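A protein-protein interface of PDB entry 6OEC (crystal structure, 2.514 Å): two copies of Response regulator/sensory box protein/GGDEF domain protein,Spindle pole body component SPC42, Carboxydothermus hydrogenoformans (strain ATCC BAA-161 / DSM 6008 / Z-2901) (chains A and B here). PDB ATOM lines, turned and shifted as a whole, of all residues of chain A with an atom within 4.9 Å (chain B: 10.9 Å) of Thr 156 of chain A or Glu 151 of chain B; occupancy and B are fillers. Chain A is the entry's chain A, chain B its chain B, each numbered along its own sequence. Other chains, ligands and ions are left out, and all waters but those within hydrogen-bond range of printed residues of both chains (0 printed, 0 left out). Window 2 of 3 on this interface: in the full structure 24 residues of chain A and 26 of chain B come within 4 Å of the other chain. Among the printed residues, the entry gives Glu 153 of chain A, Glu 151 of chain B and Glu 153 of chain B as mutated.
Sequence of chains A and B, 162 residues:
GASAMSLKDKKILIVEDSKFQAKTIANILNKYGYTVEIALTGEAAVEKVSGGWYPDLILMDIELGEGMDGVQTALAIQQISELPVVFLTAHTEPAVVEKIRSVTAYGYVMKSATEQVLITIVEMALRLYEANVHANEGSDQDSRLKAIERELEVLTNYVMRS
The backbone carbonyl oxygen (O) of Leu 152 of chain B lies close to the side-chain hydroxyl (OG1) of Thr 156 of chain B (3.2 Å).
O of Leu 152 of chain A is in hydrogen-bond range of OG1 of Thr 156 of chain A, at 3.1 Å.
Leu 152 of chain A touches just these residues of chain B: Ile 148 (3.7 Å), Leu 152 (3.6 Å) and Leu 155 (3.5 Å).
Val 159 of chain A touches two residues of chain B.
Printed residues of chain A within 4 Å of Ile 148 of chain B: Leu 152 (3.7 Å).
Of the printed residues of chain A, Glu 151 of chain B touches Thr 156.
Printed residues of chain A within 4 Å of Leu 152 of chain B: Leu 152.
Of the printed residues of chain A, Leu 155 of chain B touches Leu 152, Leu 155, Thr 156 and Val 159.
Of the printed residues of chain A, Tyr 158 of chain B touches Val 159.
The nearest residue of chain B that does not touch Thr 156 of chain A is Leu 152 of chain B (6.8 Å).
Leu 152 of chain A touches its own counterpart, Leu 152 of chain B.
Leu 152 of chain A touches Leu 155 of chain B, but with the chains exchanged Leu 155 of chain A does not touch Leu 152 of chain B (6.6 Å).
Val 159 of chain A touches Leu 155 of chain B, but with the chains exchanged Leu 155 of chain A does not touch Val 159 of chain B (9.4 Å).
Val 159 of chain A touches Tyr 158 of chain B, but with the chains exchanged Tyr 158 of chain A does not touch Val 159 of chain B (11.0 Å).
8 positions are printed for both chains.
Of the 8 pairs that touch across the chains among the printed residues, 2 have their exchanged pair printed and touching as well.
Hydrophobic or aromatic side chains of chain A within 4 Å of the printed part of chain B: Leu 152, Leu 155 and Val 159.
Hydrophobic or aromatic side chains of chain B within 4 Å of the printed part of chain A: Ile 148, Leu 152, Leu 155 and Tyr 158.
Among the printed residues, pairs that only touch across the chains: Thr 156 of chain A with Glu 151 of chain B (3.0 Å), Leu 155 of chain A with Leu 155 of chain B (3.5 Å), Leu 152 of chain A with Leu 155 of chain B (3.5 Å), Val 159 of chain A with Tyr 158 of chain B (3.6 Å), Leu 152 of chain A with Leu 152 of chain B (3.6 Å), Thr 156 of chain A with Leu 155 of chain B (3.6 Å), Leu 152 of chain A with Ile 148 of chain B (3.7 Å) and Val 159 of chain A with Leu 155 of chain B (3.8 Å).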
ATOM      1  N   LEU A 152      18.193 -33.443 -15.682  1.00  0.00           N
ATOM      2  CA  LEU A 152      19.146 -32.560 -15.018  1.00  0.00           C
ATOM      3  C   LEU A 152      20.574 -32.844 -15.470  1.00  0.00           C
ATOM      4  O   LEU A 152      21.404 -31.928 -15.493  1.00  0.00           O
ATOM      5  CB  LEU A 152      19.035 -32.691 -13.503  1.00  0.00           C
ATOM      6  CG  LEU A 152      19.997 -31.822 -12.714  1.00  0.00           C
ATOM      7  CD1 LEU A 152      19.705 -30.388 -13.028  1.00  0.00           C
ATOM      8  CD2 LEU A 152      19.903 -32.086 -11.230  1.00  0.00           C
ATOM      9  N   GLU A 153      20.877 -34.093 -15.847  1.00  0.00           N
ATOM     10  CA  GLU A 153      22.195 -34.403 -16.398  1.00  0.00           C
ATOM     11  C   GLU A 153      22.393 -33.771 -17.769  1.00  0.00           C
ATOM     12  O   GLU A 153      23.495 -33.320 -18.097  1.00  0.00           O
ATOM     13  CB  GLU A 153      22.398 -35.909 -16.506  1.00  0.00           C
ATOM     14  CG  GLU A 153      22.794 -36.607 -15.229  1.00  0.00           C
ATOM     15  CD  GLU A 153      23.191 -38.050 -15.492  1.00  0.00           C
ATOM     16  OE1 GLU A 153      24.140 -38.243 -16.300  1.00  0.00           O
ATOM     17  OE2 GLU A 153      22.538 -38.971 -14.921  1.00  0.00           O
ATOM     18  N   VAL A 154      21.357 -33.764 -18.603  1.00  0.00           N
ATOM     19  CA  VAL A 154      21.530 -33.160 -19.916  1.00  0.00           C
ATOM     20  C   VAL A 154      21.475 -31.643 -19.808  1.00  0.00           C
ATOM     21  O   VAL A 154      22.129 -30.939 -20.586  1.00  0.00           O
ATOM     22  CB  VAL A 154      20.488 -33.707 -20.911  1.00  0.00           C
ATOM     23  CG1 VAL A 154      20.501 -35.246 -20.919  1.00  0.00           C
ATOM     24  CG2 VAL A 154      19.085 -33.153 -20.616  1.00  0.00           C
ATOM     25  N   LEU A 155      20.718 -31.112 -18.841  1.00  0.00           N
ATOM     26  CA  LEU A 155      20.698 -29.667 -18.649  1.00  0.00           C
ATOM     27  C   LEU A 155      22.072 -29.161 -18.229  1.00  0.00           C
ATOM     28  O   LEU A 155      22.626 -28.255 -18.860  1.00  0.00           O
ATOM     29  CB  LEU A 155      19.635 -29.266 -17.621  1.00  0.00           C
ATOM     30  CG  LEU A 155      19.602 -27.752 -17.332  1.00  0.00           C
ATOM     31  CD1 LEU A 155      19.631 -26.926 -18.617  1.00  0.00           C
ATOM     32  CD2 LEU A 155      18.399 -27.364 -16.498  1.00  0.00           C
ATOM     33  N   THR A 156      22.647 -29.743 -17.175  1.00  0.00           N
ATOM     34  CA  THR A 156      23.934 -29.242 -16.716  1.00  0.00           C
ATOM     35  C   THR A 156      25.065 -29.611 -17.673  1.00  0.00           C
ATOM     36  O   THR A 156      26.023 -28.842 -17.805  1.00  0.00           O
ATOM     37  CB  THR A 156      24.230 -29.726 -15.299  1.00  0.00           C
ATOM     38  OG1 THR A 156      24.372 -31.144 -15.285  1.00  0.00           O
ATOM     39  CG2 THR A 156      23.105 -29.345 -14.388  1.00  0.00           C
ATOM     40  N   ASN A 157      24.983 -30.751 -18.373  1.00  0.00           N
ATOM     41  CA  ASN A 157      26.010 -31.027 -19.377  1.00  0.00           C
ATOM     42  C   ASN A 157      25.985 -29.975 -20.476  1.00  0.00           C
ATOM     43  O   ASN A 157      27.018 -29.696 -21.096  1.00  0.00           O
ATOM     44  CB  ASN A 157      25.851 -32.432 -19.980  1.00  0.00           C
ATOM     45  CG  ASN A 157      27.153 -32.945 -20.676  1.00  0.00           C
ATOM     46  OD1 ASN A 157      27.261 -32.985 -21.918  1.00  0.00           O
ATOM     47  ND2 ASN A 157      28.135 -33.335 -19.867  1.00  0.00           N
ATOM     48  N   TYR A 158      24.825 -29.363 -20.717  1.00  0.00           N
ATOM     49  CA  TYR A 158      24.747 -28.265 -21.676  1.00  0.00           C
ATOM     50  C   TYR A 158      25.304 -26.966 -21.083  1.00  0.00           C
ATOM     51  O   TYR A 158      26.009 -26.221 -21.778  1.00  0.00           O
ATOM     52  CB  TYR A 158      23.294 -28.108 -22.156  1.00  0.00           C
ATOM     53  CG  TYR A 158      22.999 -26.914 -23.058  1.00  0.00           C
ATOM     54  CD1 TYR A 158      22.713 -25.664 -22.508  1.00  0.00           C
ATOM     55  CD2 TYR A 158      22.965 -27.040 -24.446  1.00  0.00           C
ATOM     56  CE1 TYR A 158      22.429 -24.567 -23.302  1.00  0.00           C
ATOM     57  CE2 TYR A 158      22.676 -25.938 -25.259  1.00  0.00           C
ATOM     58  CZ  TYR A 158      22.406 -24.701 -24.669  1.00  0.00           C
ATOM     59  OH  TYR A 158      22.111 -23.578 -25.418  1.00  0.00           O
ATOM     60  N   VAL A 159      25.032 -26.691 -19.799  1.00  0.00           N
ATOM     61  CA  VAL A 159      25.629 -25.519 -19.151  1.00  0.00           C
ATOM     62  C   VAL A 159      27.142 -25.673 -19.058  1.00  0.00           C
ATOM     63  O   VAL A 159      27.886 -24.696 -19.209  1.00  0.00           O
ATOM     64  CB  VAL A 159      25.010 -25.271 -17.757  1.00  0.00           C
ATOM     65  CG1 VAL A 159      25.599 -24.007 -17.123  1.00  0.00           C
ATOM     66  CG2 VAL A 159      23.493 -25.172 -17.855  1.00  0.00           C
ATOM     67  N   MET A 160      27.624 -26.902 -18.860  1.00  0.00           N
ATOM     68  CA  MET A 160      29.053 -27.190 -18.810  1.00  0.00           C
ATOM     69  C   MET A 160      29.758 -26.881 -20.133  1.00  0.00           C
ATOM     70  O   MET A 160      30.902 -27.302 -20.334  1.00  0.00           O
ATOM     71  CB  MET A 160      29.266 -28.655 -18.429  1.00  0.00           C
ATOM     72  CG  MET A 160      30.415 -28.891 -17.480  1.00  0.00           C
ATOM     73  SD  MET A 160      30.059 -28.245 -15.844  1.00  0.00           S
ATOM     74  CE  MET A 160      31.422 -28.931 -14.930  1.00  0.00           C
ATOM     75  N   SER B 143      19.467 -39.646  -0.644  1.00  0.00           N
ATOM     76  CA  SER B 143      20.776 -39.094  -0.985  1.00  0.00           C
ATOM     77  C   SER B 143      20.789 -38.556  -2.408  1.00  0.00           C
ATOM     78  O   SER B 143      21.509 -37.596  -2.707  1.00  0.00           O
ATOM     79  CB  SER B 143      21.868 -40.143  -0.789  1.00  0.00           C
ATOM     80  OG  SER B 143      22.026 -40.472   0.589  1.00  0.00           O
ATOM     81  N   ARG B 144      19.994 -39.156  -3.294  1.00  0.00           N
ATOM     82  CA  ARG B 144      19.803 -38.580  -4.618  1.00  0.00           C
ATOM     83  C   ARG B 144      19.083 -37.245  -4.525  1.00  0.00           C
ATOM     84  O   ARG B 144      19.388 -36.315  -5.279  1.00  0.00           O
ATOM     85  CB  ARG B 144      19.030 -39.563  -5.498  1.00  0.00           C
ATOM     86  CG  ARG B 144      19.760 -40.885  -5.705  1.00  0.00           C
ATOM     87  CD  ARG B 144      18.802 -42.066  -5.821  1.00  0.00           C
ATOM     88  NE  ARG B 144      18.033 -42.043  -7.063  1.00  0.00           N
ATOM     89  CZ  ARG B 144      17.244 -43.034  -7.477  1.00  0.00           C
ATOM     90  NH1 ARG B 144      16.587 -42.911  -8.630  1.00  0.00           N
ATOM     91  NH2 ARG B 144      17.114 -44.147  -6.745  1.00  0.00           N
ATOM     92  N   LEU B 145      18.140 -37.126  -3.587  1.00  0.00           N
ATOM     93  CA  LEU B 145      17.399 -35.878  -3.427  1.00  0.00           C
ATOM     94  C   LEU B 145      18.311 -34.730  -3.004  1.00  0.00           C
ATOM     95  O   LEU B 145      18.214 -33.616  -3.541  1.00  0.00           O
ATOM     96  CB  LEU B 145      16.263 -36.069  -2.422  1.00  0.00           C
ATOM     97  CG  LEU B 145      15.008 -36.690  -3.038  1.00  0.00           C
ATOM     98  CD1 LEU B 145      13.950 -36.938  -1.977  1.00  0.00           C
ATOM     99  CD2 LEU B 145      14.460 -35.789  -4.143  1.00  0.00           C
ATOM    100  N   LYS B 146      19.204 -34.981  -2.044  1.00  0.00           N
ATOM    101  CA  LYS B 146      20.138 -33.941  -1.622  1.00  0.00           C
ATOM    102  C   LYS B 146      20.933 -33.417  -2.812  1.00  0.00           C
ATOM    103  O   LYS B 146      21.014 -32.201  -3.042  1.00  0.00           O
ATOM    104  CB  LYS B 146      21.077 -34.476  -0.537  1.00  0.00           C
ATOM    105  CG  LYS B 146      20.656 -35.822   0.034  1.00  0.00           C
ATOM    106  CD  LYS B 146      21.171 -36.082   1.450  1.00  0.00           C
ATOM    107  CE  LYS B 146      20.515 -37.331   2.053  1.00  0.00           C
ATOM    108  NZ  LYS B 146      20.774 -37.484   3.514  1.00  0.00           N
ATOM    109  N   ALA B 147      21.496 -34.328  -3.605  1.00  0.00           N
ATOM    110  CA  ALA B 147      22.341 -33.914  -4.716  1.00  0.00           C
ATOM    111  C   ALA B 147      21.538 -33.167  -5.766  1.00  0.00           C
ATOM    112  O   ALA B 147      21.989 -32.145  -6.291  1.00  0.00           O
ATOM    113  CB  ALA B 147      23.025 -35.136  -5.324  1.00  0.00           C
ATOM    114  N   ILE B 148      20.335 -33.651  -6.067  1.00  0.00           N
ATOM    115  CA  ILE B 148      19.536 -33.049  -7.127  1.00  0.00           C
ATOM    116  C   ILE B 148      19.067 -31.657  -6.716  1.00  0.00           C
ATOM    117  O   ILE B 148      19.015 -30.733  -7.540  1.00  0.00           O
ATOM    118  CB  ILE B 148      18.369 -33.988  -7.490  1.00  0.00           C
ATOM    119  CG1 ILE B 148      17.648 -33.546  -8.750  1.00  0.00           C
ATOM    120  CG2 ILE B 148      17.353 -34.064  -6.394  1.00  0.00           C
ATOM    121  CD1 ILE B 148      16.541 -34.502  -9.074  1.00  0.00           C
ATOM    122  N   GLU B 149      18.761 -31.470  -5.431  1.00  0.00           N
ATOM    123  CA  GLU B 149      18.399 -30.138  -4.977  1.00  0.00           C
ATOM    124  C   GLU B 149      19.616 -29.224  -4.948  1.00  0.00           C
ATOM    125  O   GLU B 149      19.537 -28.061  -5.363  1.00  0.00           O
ATOM    126  CB  GLU B 149      17.732 -30.218  -3.601  1.00  0.00           C
ATOM    127  CG  GLU B 149      16.231 -30.509  -3.660  1.00  0.00           C
ATOM    128  CD  GLU B 149      15.552 -30.406  -2.307  1.00  0.00           C
ATOM    129  OE1 GLU B 149      15.936 -31.172  -1.397  1.00  0.00           O
ATOM    130  OE2 GLU B 149      14.642 -29.553  -2.157  1.00  0.00           O
ATOM    131  N   ARG B 150      20.756 -29.751  -4.489  1.00  0.00           N
ATOM    132  CA  ARG B 150      21.975 -28.952  -4.378  1.00  0.00           C
ATOM    133  C   ARG B 150      22.442 -28.432  -5.736  1.00  0.00           C
ATOM    134  O   ARG B 150      22.881 -27.280  -5.854  1.00  0.00           O
ATOM    135  CB  ARG B 150      23.074 -29.782  -3.718  1.00  0.00           C
ATOM    136  CG  ARG B 150      23.914 -28.997  -2.731  1.00  0.00           C
ATOM    137  CD  ARG B 150      24.820 -27.966  -3.427  1.00  0.00           C
ATOM    138  NE  ARG B 150      25.762 -27.361  -2.483  1.00  0.00           N
ATOM    139  CZ  ARG B 150      26.797 -28.000  -1.931  1.00  0.00           C
ATOM    140  NH1 ARG B 150      27.048 -29.277  -2.229  1.00  0.00           N
ATOM    141  NH2 ARG B 150      27.589 -27.357  -1.080  1.00  0.00           N
ATOM    142  N   GLU B 151      22.377 -29.278  -6.766  1.00  0.00           N
ATOM    143  CA  GLU B 151      22.744 -28.834  -8.100  1.00  0.00           C
ATOM    144  C   GLU B 151      21.718 -27.871  -8.659  1.00  0.00           C
ATOM    145  O   GLU B 151      22.067 -27.000  -9.462  1.00  0.00           O
ATOM    146  CB  GLU B 151      22.913 -30.030  -9.040  1.00  0.00           C
ATOM    147  CG  GLU B 151      23.150 -29.672 -10.523  1.00  0.00           C
ATOM    148  CD  GLU B 151      24.479 -28.952 -10.797  1.00  0.00           C
ATOM    149  OE1 GLU B 151      24.658 -28.467 -11.933  1.00  0.00           O
ATOM    150  OE2 GLU B 151      25.342 -28.873  -9.894  1.00  0.00           O
ATOM    151  N   LEU B 152      20.454 -28.001  -8.257  1.00  0.00           N
ATOM    152  CA  LEU B 152      19.479 -27.038  -8.754  1.00  0.00           C
ATOM    153  C   LEU B 152      19.734 -25.650  -8.177  1.00  0.00           C
ATOM    154  O   LEU B 152      19.522 -24.650  -8.869  1.00  0.00           O
ATOM    155  CB  LEU B 152      18.055 -27.508  -8.474  1.00  0.00           C
ATOM    156  CG  LEU B 152      17.388 -27.906  -9.790  1.00  0.00           C
ATOM    157  CD1 LEU B 152      17.801 -29.296 -10.173  1.00  0.00           C
ATOM    158  CD2 LEU B 152      15.890 -27.820  -9.706  1.00  0.00           C
ATOM    159  N   GLU B 153      20.227 -25.565  -6.938  1.00  0.00           N
ATOM    160  CA  GLU B 153      20.686 -24.279  -6.416  1.00  0.00           C
ATOM    161  C   GLU B 153      21.803 -23.715  -7.280  1.00  0.00           C
ATOM    162  O   GLU B 153      21.685 -22.622  -7.849  1.00  0.00           O
ATOM    163  CB  GLU B 153      21.169 -24.426  -4.973  1.00  0.00           C
ATOM    164  CG  GLU B 153      21.996 -23.242  -4.515  1.00  0.00           C
ATOM    165  CD  GLU B 153      22.427 -23.359  -3.071  1.00  0.00           C
ATOM    166  OE1 GLU B 153      22.507 -22.307  -2.384  1.00  0.00           O
ATOM    167  OE2 GLU B 153      22.679 -24.507  -2.632  1.00  0.00           O
ATOM    168  N   VAL B 154      22.906 -24.459  -7.369  1.00  0.00           N
ATOM    169  CA  VAL B 154      24.053 -24.162  -8.215  1.00  0.00           C
ATOM    170  C   VAL B 154      23.598 -23.754  -9.604  1.00  0.00           C
ATOM    171  O   VAL B 154      24.001 -22.708 -10.123  1.00  0.00           O
ATOM    172  CB  VAL B 154      24.979 -25.384  -8.301  1.00  0.00           C
ATOM    173  CG1 VAL B 154      26.114 -25.134  -9.313  1.00  0.00           C
ATOM    174  CG2 VAL B 154      25.493 -25.759  -6.909  1.00  0.00           C
ATOM    175  N   LEU B 155      22.777 -24.602 -10.220  1.00  0.00           N
ATOM    176  CA  LEU B 155      22.252 -24.301 -11.544  1.00  0.00           C
ATOM    177  C   LEU B 155      21.489 -22.986 -11.536  1.00  0.00           C
ATOM    178  O   LEU B 155      21.609 -22.185 -12.471  1.00  0.00           O
ATOM    179  CB  LEU B 155      21.357 -25.450 -12.005  1.00  0.00           C
ATOM    180  CG  LEU B 155      21.129 -25.667 -13.493  1.00  0.00           C
ATOM    181  CD1 LEU B 155      22.450 -25.667 -14.229  1.00  0.00           C
ATOM    182  CD2 LEU B 155      20.421 -26.981 -13.684  1.00  0.00           C
ATOM    183  N   THR B 156      20.719 -22.734 -10.468  1.00  0.00           N
ATOM    184  CA  THR B 156      19.876 -21.540 -10.408  1.00  0.00           C
ATOM    185  C   THR B 156      20.733 -20.279 -10.348  1.00  0.00           C
ATOM    186  O   THR B 156      20.571 -19.368 -11.174  1.00  0.00           O
ATOM    187  CB  THR B 156      18.901 -21.644  -9.216  1.00  0.00           C
ATOM    188  OG1 THR B 156      17.648 -22.199  -9.658  1.00  0.00           O
ATOM    189  CG2 THR B 156      18.638 -20.290  -8.545  1.00  0.00           C
ATOM    190  N   ASN B 157      21.697 -20.240  -9.419  1.00  0.00           N
ATOM    191  CA  ASN B 157      22.578 -19.083  -9.278  1.00  0.00           C
ATOM    192  C   ASN B 157      23.203 -18.650 -10.603  1.00  0.00           C
ATOM    193  O   ASN B 157      23.563 -17.478 -10.753  1.00  0.00           O
ATOM    194  CB  ASN B 157      23.674 -19.391  -8.243  1.00  0.00           C
ATOM    195  CG  ASN B 157      23.102 -19.872  -6.911  1.00  0.00           C
ATOM    196  OD1 ASN B 157      21.892 -19.822  -6.699  1.00  0.00           O
ATOM    197  ND2 ASN B 157      23.968 -20.328  -6.008  1.00  0.00           N
ATOM    198  N   TYR B 158      23.296 -19.553 -11.585  1.00  0.00           N
ATOM    199  CA  TYR B 158      23.979 -19.261 -12.841  1.00  0.00           C
ATOM    200  C   TYR B 158      23.269 -18.206 -13.687  1.00  0.00           C
ATOM    201  O   TYR B 158      23.828 -17.764 -14.698  1.00  0.00           O
ATOM    202  CB  TYR B 158      24.164 -20.561 -13.636  1.00  0.00           C
ATOM    203  CG  TYR B 158      24.726 -20.393 -15.035  1.00  0.00           C
ATOM    204  CD1 TYR B 158      23.999 -20.799 -16.147  1.00  0.00           C
ATOM    205  CD2 TYR B 158      25.964 -19.813 -15.249  1.00  0.00           C
ATOM    206  CE1 TYR B 158      24.492 -20.645 -17.432  1.00  0.00           C
ATOM    207  CE2 TYR B 158      26.460 -19.652 -16.534  1.00  0.00           C
ATOM    208  CZ  TYR B 158      25.714 -20.072 -17.616  1.00  0.00           C
ATOM    209  OH  TYR B 158      26.187 -19.926 -18.891  1.00  0.00           O
ATOM    210  N   VAL B 159      22.083 -17.756 -13.302  1.00  0.00           N
ATOM    211  CA  VAL B 159      21.434 -16.664 -14.017  1.00  0.00           C
ATOM    212  C   VAL B 159      21.786 -15.346 -13.326  1.00  0.00           C
ATOM    213  O   VAL B 159      21.488 -15.152 -12.138  1.00  0.00           O
ATOM    214  CB  VAL B 159      19.919 -16.881 -14.111  1.00  0.00           C
ATOM    215  CG1 VAL B 159      19.285 -15.781 -14.941  1.00  0.00           C
ATOM    216  CG2 VAL B 159      19.643 -18.243 -14.737  1.00  0.00           C
